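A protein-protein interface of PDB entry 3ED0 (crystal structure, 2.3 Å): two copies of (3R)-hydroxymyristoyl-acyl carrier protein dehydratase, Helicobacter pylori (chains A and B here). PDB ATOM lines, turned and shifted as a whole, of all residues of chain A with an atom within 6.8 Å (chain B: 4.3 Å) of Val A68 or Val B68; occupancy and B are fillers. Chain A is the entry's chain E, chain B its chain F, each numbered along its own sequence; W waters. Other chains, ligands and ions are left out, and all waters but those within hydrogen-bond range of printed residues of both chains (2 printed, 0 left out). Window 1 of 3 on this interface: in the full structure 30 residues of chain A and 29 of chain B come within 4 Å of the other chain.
Printed residues of chain A that touch a printed residue of chain B: Met A27, Val A68, Glu A72, Phe A101 and Phe A109. Hydrophobic or aromatic side chains of chain A that line the printed part of chain B: Met A27, Val A68, Phe A101 and Phe A109. Of the 8 printed residues of chain B, 4 touch a printed residue of chain A.
Water W1 lies within hydrogen-bond range of OE1 of Glu B72 (2.5 Å), N of Val A68 (3.0 Å) and N of Gly A67 (3.1 Å). Water W2 lies within hydrogen-bond range of OE1 of Glu A72, N of Gly B67 and N of Val B68.
Of the printed residues of chain B, Met A27 touches Pro B66 (3.8 Å). Val A68 touches just these residues of chain B: Val B68 (3.6 Å), Glu B72 (3.5 Å) and Phe B101 (3.7 Å). Of the printed residues of chain B, Phe A101 touches Val B68. Of the printed residues of chain B, Phe A109 touches Phe B101 (3.4 Å). Of chain A, only Val A68, Glu A72 and Phe A101 come within 4 Å of Val B68. Of the printed residues of chain A, Phe B101 touches Val A68 (3.7 Å) and Phe A109 (3.4 Å).
Val B68 touches its own counterpart, Val A68. Val A68 touches Glu B72, and with the chains exchanged Glu A72 touches Val B68. Val A68 touches Phe B101, and with the chains exchanged Phe A101 touches Val B68. 8 positions are printed for both chains. Of the 7 pairs that touch across the chains among the printed residues, 5 have their exchanged pair printed and touching as well.
Among the printed residues, merely in contact across the chains: Met A27 with Pro B66 (3.8 Å), Val A68 with Val B68 (3.6 Å), Val A68 with Glu B72 (3.5 Å), Val A68 with Phe B101 (3.7 Å), Glu A72 with Val B68 (3.6 Å), Phe A101 with Val B68 (3.6 Å) and Phe A109 with Phe B101 (3.4 Å).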
ATOM      1  N   MET A  27      25.909  19.835 -27.819  1.00  0.00           N
ATOM      2  CA  MET A  27      25.366  19.573 -26.487  1.00  0.00           C
ATOM      3  C   MET A  27      23.976  18.921 -26.405  1.00  0.00           C
ATOM      4  O   MET A  27      23.312  18.995 -25.369  1.00  0.00           O
ATOM      5  CB  MET A  27      25.374  20.862 -25.672  1.00  0.00           C
ATOM      6  CG  MET A  27      26.751  21.259 -25.172  1.00  0.00           C
ATOM      7  SD  MET A  27      27.421  20.085 -23.953  1.00  0.00           S
ATOM      8  CE  MET A  27      26.299  20.382 -22.588  1.00  0.00           C
ATOM      9  N   LEU A  29      22.580  15.612 -26.158  1.00  0.00           N
ATOM     10  CA  LEU A  29      23.059  14.271 -25.865  1.00  0.00           C
ATOM     11  C   LEU A  29      22.018  13.159 -25.707  1.00  0.00           C
ATOM     12  O   LEU A  29      22.198  12.232 -24.918  1.00  0.00           O
ATOM     13  CB  LEU A  29      23.966  14.340 -24.625  1.00  0.00           C
ATOM     14  CG  LEU A  29      25.012  15.472 -24.691  1.00  0.00           C
ATOM     15  CD1 LEU A  29      25.886  15.457 -23.444  1.00  0.00           C
ATOM     16  CD2 LEU A  29      25.874  15.316 -25.940  1.00  0.00           C
ATOM     17  N   PHE A  65      33.885   8.360 -22.518  1.00  0.00           N
ATOM     18  CA  PHE A  65      32.829   9.363 -22.502  1.00  0.00           C
ATOM     19  C   PHE A  65      32.811  10.026 -21.124  1.00  0.00           C
ATOM     20  O   PHE A  65      32.693   9.346 -20.112  1.00  0.00           O
ATOM     21  CB  PHE A  65      31.480   8.716 -22.792  1.00  0.00           C
ATOM     22  CG  PHE A  65      30.421   9.695 -23.207  1.00  0.00           C
ATOM     23  CD1 PHE A  65      30.520  10.368 -24.420  1.00  0.00           C
ATOM     24  CD2 PHE A  65      29.328   9.949 -22.385  1.00  0.00           C
ATOM     25  CE1 PHE A  65      29.549  11.276 -24.806  1.00  0.00           C
ATOM     26  CE2 PHE A  65      28.349  10.856 -22.762  1.00  0.00           C
ATOM     27  CZ  PHE A  65      28.461  11.521 -23.978  1.00  0.00           C
ATOM     28  N   PRO A  66      32.931  11.365 -21.071  1.00  0.00           N
ATOM     29  CA  PRO A  66      32.936  12.101 -19.799  1.00  0.00           C
ATOM     30  C   PRO A  66      31.736  11.823 -18.896  1.00  0.00           C
ATOM     31  O   PRO A  66      30.585  11.889 -19.337  1.00  0.00           O
ATOM     32  CB  PRO A  66      32.997  13.566 -20.240  1.00  0.00           C
ATOM     33  CG  PRO A  66      33.702  13.509 -21.557  1.00  0.00           C
ATOM     34  CD  PRO A  66      33.072  12.294 -22.210  1.00  0.00           C
ATOM     35  N   GLY A  67      32.024  11.512 -17.633  1.00  0.00           N
ATOM     36  CA  GLY A  67      30.979  11.249 -16.665  1.00  0.00           C
ATOM     37  C   GLY A  67      29.998  12.406 -16.564  1.00  0.00           C
ATOM     38  O   GLY A  67      28.785  12.188 -16.470  1.00  0.00           O
ATOM     39  N   VAL A  68      30.510  13.636 -16.596  1.00  0.00           N
ATOM     40  CA  VAL A  68      29.639  14.806 -16.508  1.00  0.00           C
ATOM     41  C   VAL A  68      28.678  14.910 -17.689  1.00  0.00           C
ATOM     42  O   VAL A  68      27.589  15.459 -17.556  1.00  0.00           O
ATOM     43  CB  VAL A  68      30.433  16.141 -16.400  1.00  0.00           C
ATOM     44  CG1 VAL A  68      31.236  16.164 -15.121  1.00  0.00           C
ATOM     45  CG2 VAL A  68      31.324  16.333 -17.608  1.00  0.00           C
ATOM     46  N   LEU A  69      29.059  14.376 -18.843  1.00  0.00           N
ATOM     47  CA  LEU A  69      28.168  14.441 -19.995  1.00  0.00           C
ATOM     48  C   LEU A  69      27.087  13.370 -19.899  1.00  0.00           C
ATOM     49  O   LEU A  69      26.026  13.502 -20.503  1.00  0.00           O
ATOM     50  CB  LEU A  69      28.953  14.320 -21.309  1.00  0.00           C
ATOM     51  CG  LEU A  69      29.864  15.519 -21.626  1.00  0.00           C
ATOM     52  CD1 LEU A  69      30.451  15.386 -23.034  1.00  0.00           C
ATOM     53  CD2 LEU A  69      29.071  16.814 -21.511  1.00  0.00           C
ATOM     54  N   ILE A  70      27.362  12.308 -19.141  1.00  0.00           N
ATOM     55  CA  ILE A  70      26.384  11.240 -18.927  1.00  0.00           C
ATOM     56  C   ILE A  70      25.256  11.859 -18.101  1.00  0.00           C
ATOM     57  O   ILE A  70      24.074  11.621 -18.355  1.00  0.00           O
ATOM     58  CB  ILE A  70      26.976  10.069 -18.116  1.00  0.00           C
ATOM     59  CG1 ILE A  70      28.026   9.325 -18.942  1.00  0.00           C
ATOM     60  CG2 ILE A  70      25.854   9.120 -17.690  1.00  0.00           C
ATOM     61  CD1 ILE A  70      28.722   8.195 -18.194  1.00  0.00           C
ATOM     62  N   VAL A  71      25.644  12.653 -17.106  1.00  0.00           N
ATOM     63  CA  VAL A  71      24.694  13.338 -16.240  1.00  0.00           C
ATOM     64  C   VAL A  71      23.877  14.313 -17.077  1.00  0.00           C
ATOM     65  O   VAL A  71      22.657  14.407 -16.931  1.00  0.00           O
ATOM     66  CB  VAL A  71      25.418  14.140 -15.143  1.00  0.00           C
ATOM     67  CG1 VAL A  71      24.406  14.923 -14.315  1.00  0.00           C
ATOM     68  CG2 VAL A  71      26.217  13.206 -14.266  1.00  0.00           C
ATOM     69  N   GLU A  72      24.570  15.038 -17.949  1.00  0.00           N
ATOM     70  CA  GLU A  72      23.926  16.001 -18.830  1.00  0.00           C
ATOM     71  C   GLU A  72      22.884  15.281 -19.682  1.00  0.00           C
ATOM     72  O   GLU A  72      21.798  15.808 -19.921  1.00  0.00           O
ATOM     73  CB  GLU A  72      24.975  16.675 -19.719  1.00  0.00           C
ATOM     74  CG  GLU A  72      24.430  17.662 -20.755  1.00  0.00           C
ATOM     75  CD  GLU A  72      23.749  18.883 -20.142  1.00  0.00           C
ATOM     76  OE1 GLU A  72      24.192  19.350 -19.070  1.00  0.00           O
ATOM     77  OE2 GLU A  72      22.781  19.388 -20.748  1.00  0.00           O
ATOM     78  N   GLY A  73      23.218  14.073 -20.128  1.00  0.00           N
ATOM     79  CA  GLY A  73      22.295  13.301 -20.940  1.00  0.00           C
ATOM     80  C   GLY A  73      21.063  12.890 -20.145  1.00  0.00           C
ATOM     81  O   GLY A  73      19.948  12.856 -20.671  1.00  0.00           O
ATOM     82  N   ALA A  75      19.879  14.554 -17.563  1.00  0.00           N
ATOM     83  CA  ALA A  75      19.132  15.776 -17.305  1.00  0.00           C
ATOM     84  C   ALA A  75      18.283  16.119 -18.518  1.00  0.00           C
ATOM     85  O   ALA A  75      17.121  16.497 -18.389  1.00  0.00           O
ATOM     86  CB  ALA A  75      20.086  16.915 -16.991  1.00  0.00           C
ATOM     87  N   PHE A 101      20.186  23.842 -14.932  1.00  0.00           N
ATOM     88  CA  PHE A 101      20.490  22.842 -13.928  1.00  0.00           C
ATOM     89  C   PHE A 101      20.385  23.585 -12.595  1.00  0.00           C
ATOM     90  O   PHE A 101      20.839  24.723 -12.489  1.00  0.00           O
ATOM     91  CB  PHE A 101      21.925  22.352 -14.114  1.00  0.00           C
ATOM     92  CG  PHE A 101      22.042  20.878 -14.320  1.00  0.00           C
ATOM     93  CD1 PHE A 101      21.636  19.992 -13.331  1.00  0.00           C
ATOM     94  CD2 PHE A 101      22.562  20.371 -15.505  1.00  0.00           C
ATOM     95  CE1 PHE A 101      21.749  18.614 -13.519  1.00  0.00           C
ATOM     96  CE2 PHE A 101      22.679  18.998 -15.704  1.00  0.00           C
ATOM     97  CZ  PHE A 101      22.271  18.116 -14.708  1.00  0.00           C
ATOM     98  N   ILE A 104      22.656  18.804  -8.321  1.00  0.00           N
ATOM     99  CA  ILE A 104      23.078  17.468  -8.716  1.00  0.00           C
ATOM    100  C   ILE A 104      23.478  16.775  -7.424  1.00  0.00           C
ATOM    101  O   ILE A 104      24.197  17.351  -6.614  1.00  0.00           O
ATOM    102  CB  ILE A 104      24.306  17.509  -9.657  1.00  0.00           C
ATOM    103  CG1 ILE A 104      23.989  18.333 -10.905  1.00  0.00           C
ATOM    104  CG2 ILE A 104      24.709  16.096 -10.051  1.00  0.00           C
ATOM    105  CD1 ILE A 104      25.163  18.492 -11.836  1.00  0.00           C
ATOM    106  N   PHE A 109      29.693   6.873 -10.468  1.00  0.00           N
ATOM    107  CA  PHE A 109      30.057   6.261 -11.746  1.00  0.00           C
ATOM    108  C   PHE A 109      30.651   4.893 -11.428  1.00  0.00           C
ATOM    109  O   PHE A 109      31.566   4.789 -10.622  1.00  0.00           O
ATOM    110  CB  PHE A 109      31.075   7.138 -12.489  1.00  0.00           C
ATOM    111  CG  PHE A 109      30.584   8.537 -12.766  1.00  0.00           C
ATOM    112  CD1 PHE A 109      31.071   9.621 -12.042  1.00  0.00           C
ATOM    113  CD2 PHE A 109      29.623   8.771 -13.746  1.00  0.00           C
ATOM    114  CE1 PHE A 109      30.607  10.921 -12.292  1.00  0.00           C
ATOM    115  CE2 PHE A 109      29.156  10.064 -14.000  1.00  0.00           C
ATOM    116  CZ  PHE A 109      29.650  11.137 -13.273  1.00  0.00           C
ATOM    117  N   PRO B  66      27.846  25.367 -19.665  1.00  0.00           N
ATOM    118  CA  PRO B  66      27.181  24.237 -19.001  1.00  0.00           C
ATOM    119  C   PRO B  66      27.572  23.964 -17.550  1.00  0.00           C
ATOM    120  O   PRO B  66      28.750  23.843 -17.213  1.00  0.00           O
ATOM    121  CB  PRO B  66      27.504  23.054 -19.922  1.00  0.00           C
ATOM    122  CG  PRO B  66      27.649  23.703 -21.269  1.00  0.00           C
ATOM    123  CD  PRO B  66      28.468  24.927 -20.927  1.00  0.00           C
ATOM    124  N   GLY B  67      26.559  23.855 -16.699  1.00  0.00           N
ATOM    125  CA  GLY B  67      26.802  23.580 -15.297  1.00  0.00           C
ATOM    126  C   GLY B  67      27.681  22.358 -15.098  1.00  0.00           C
ATOM    127  O   GLY B  67      28.557  22.354 -14.239  1.00  0.00           O
ATOM    128  N   VAL B  68      27.455  21.317 -15.895  1.00  0.00           N
ATOM    129  CA  VAL B  68      28.244  20.110 -15.758  1.00  0.00           C
ATOM    130  C   VAL B  68      29.707  20.346 -16.108  1.00  0.00           C
ATOM    131  O   VAL B  68      30.587  19.645 -15.604  1.00  0.00           O
ATOM    132  CB  VAL B  68      27.685  18.953 -16.623  1.00  0.00           C
ATOM    133  CG1 VAL B  68      26.268  18.639 -16.197  1.00  0.00           C
ATOM    134  CG2 VAL B  68      27.744  19.305 -18.094  1.00  0.00           C
ATOM    135  N   LEU B  69      29.965  21.338 -16.959  1.00  0.00           N
ATOM    136  CA  LEU B  69      31.333  21.643 -17.352  1.00  0.00           C
ATOM    137  C   LEU B  69      32.009  22.471 -16.277  1.00  0.00           C
ATOM    138  O   LEU B  69      33.235  22.489 -16.179  1.00  0.00           O
ATOM    139  CB  LEU B  69      31.365  22.354 -18.707  1.00  0.00           C
ATOM    140  CG  LEU B  69      30.965  21.431 -19.871  1.00  0.00           C
ATOM    141  CD1 LEU B  69      31.228  22.124 -21.193  1.00  0.00           C
ATOM    142  CD2 LEU B  69      31.755  20.120 -19.790  1.00  0.00           C
ATOM    143  N   ILE B  70      31.204  23.156 -15.468  1.00  0.00           N
ATOM    144  CA  ILE B  70      31.744  23.927 -14.362  1.00  0.00           C
ATOM    145  C   ILE B  70      32.263  22.886 -13.377  1.00  0.00           C
ATOM    146  O   ILE B  70      33.371  23.002 -12.858  1.00  0.00           O
ATOM    147  CB  ILE B  70      30.668  24.776 -13.661  1.00  0.00           C
ATOM    148  CG1 ILE B  70      30.117  25.828 -14.630  1.00  0.00           C
ATOM    149  CG2 ILE B  70      31.266  25.464 -12.434  1.00  0.00           C
ATOM    150  CD1 ILE B  70      29.023  26.692 -14.052  1.00  0.00           C
ATOM    151  N   VAL B  71      31.455  21.861 -13.129  1.00  0.00           N
ATOM    152  CA  VAL B  71      31.847  20.792 -12.220  1.00  0.00           C
ATOM    153  C   VAL B  71      33.100  20.086 -12.754  1.00  0.00           C
ATOM    154  O   VAL B  71      34.004  19.764 -11.988  1.00  0.00           O
ATOM    155  CB  VAL B  71      30.707  19.749 -12.043  1.00  0.00           C
ATOM    156  CG1 VAL B  71      31.189  18.583 -11.185  1.00  0.00           C
ATOM    157  CG2 VAL B  71      29.490  20.406 -11.403  1.00  0.00           C
ATOM    158  N   GLU B  72      33.143  19.852 -14.066  1.00  0.00           N
ATOM    159  CA  GLU B  72      34.288  19.199 -14.701  1.00  0.00           C
ATOM    160  C   GLU B  72      35.555  20.013 -14.430  1.00  0.00           C
ATOM    161  O   GLU B  72      36.607  19.462 -14.094  1.00  0.00           O
ATOM    162  CB  GLU B  72      34.046  19.068 -16.214  1.00  0.00           C
ATOM    163  CG  GLU B  72      35.176  18.413 -17.016  1.00  0.00           C
ATOM    164  CD  GLU B  72      35.534  17.000 -16.548  1.00  0.00           C
ATOM    165  OE1 GLU B  72      34.622  16.225 -16.183  1.00  0.00           O
ATOM    166  OE2 GLU B  72      36.734  16.656 -16.562  1.00  0.00           O
ATOM    167  N   PHE B 101      36.083  10.011 -12.897  1.00  0.00           N
ATOM    168  CA  PHE B 101      35.163  10.614 -11.952  1.00  0.00           C
ATOM    169  C   PHE B 101      34.582   9.424 -11.191  1.00  0.00           C
ATOM    170  O   PHE B 101      34.251   8.413 -11.812  1.00  0.00           O
ATOM    171  CB  PHE B 101      34.040  11.324 -12.700  1.00  0.00           C
ATOM    172  CG  PHE B 101      33.905  12.780 -12.360  1.00  0.00           C
ATOM    173  CD1 PHE B 101      34.258  13.756 -13.285  1.00  0.00           C
ATOM    174  CD2 PHE B 101      33.401  13.175 -11.128  1.00  0.00           C
ATOM    175  CE1 PHE B 101      34.107  15.101 -12.987  1.00  0.00           C
ATOM    176  CE2 PHE B 101      33.245  14.520 -10.821  1.00  0.00           C
ATOM    177  CZ  PHE B 101      33.598  15.485 -11.751  1.00  0.00           C
HETATM  178  O   HOH W   1      33.474  14.089 -16.789  1.00  0.00           O
HETATM  179  O   HOH W   2      25.043  21.487 -17.952  1.00  0.00           O
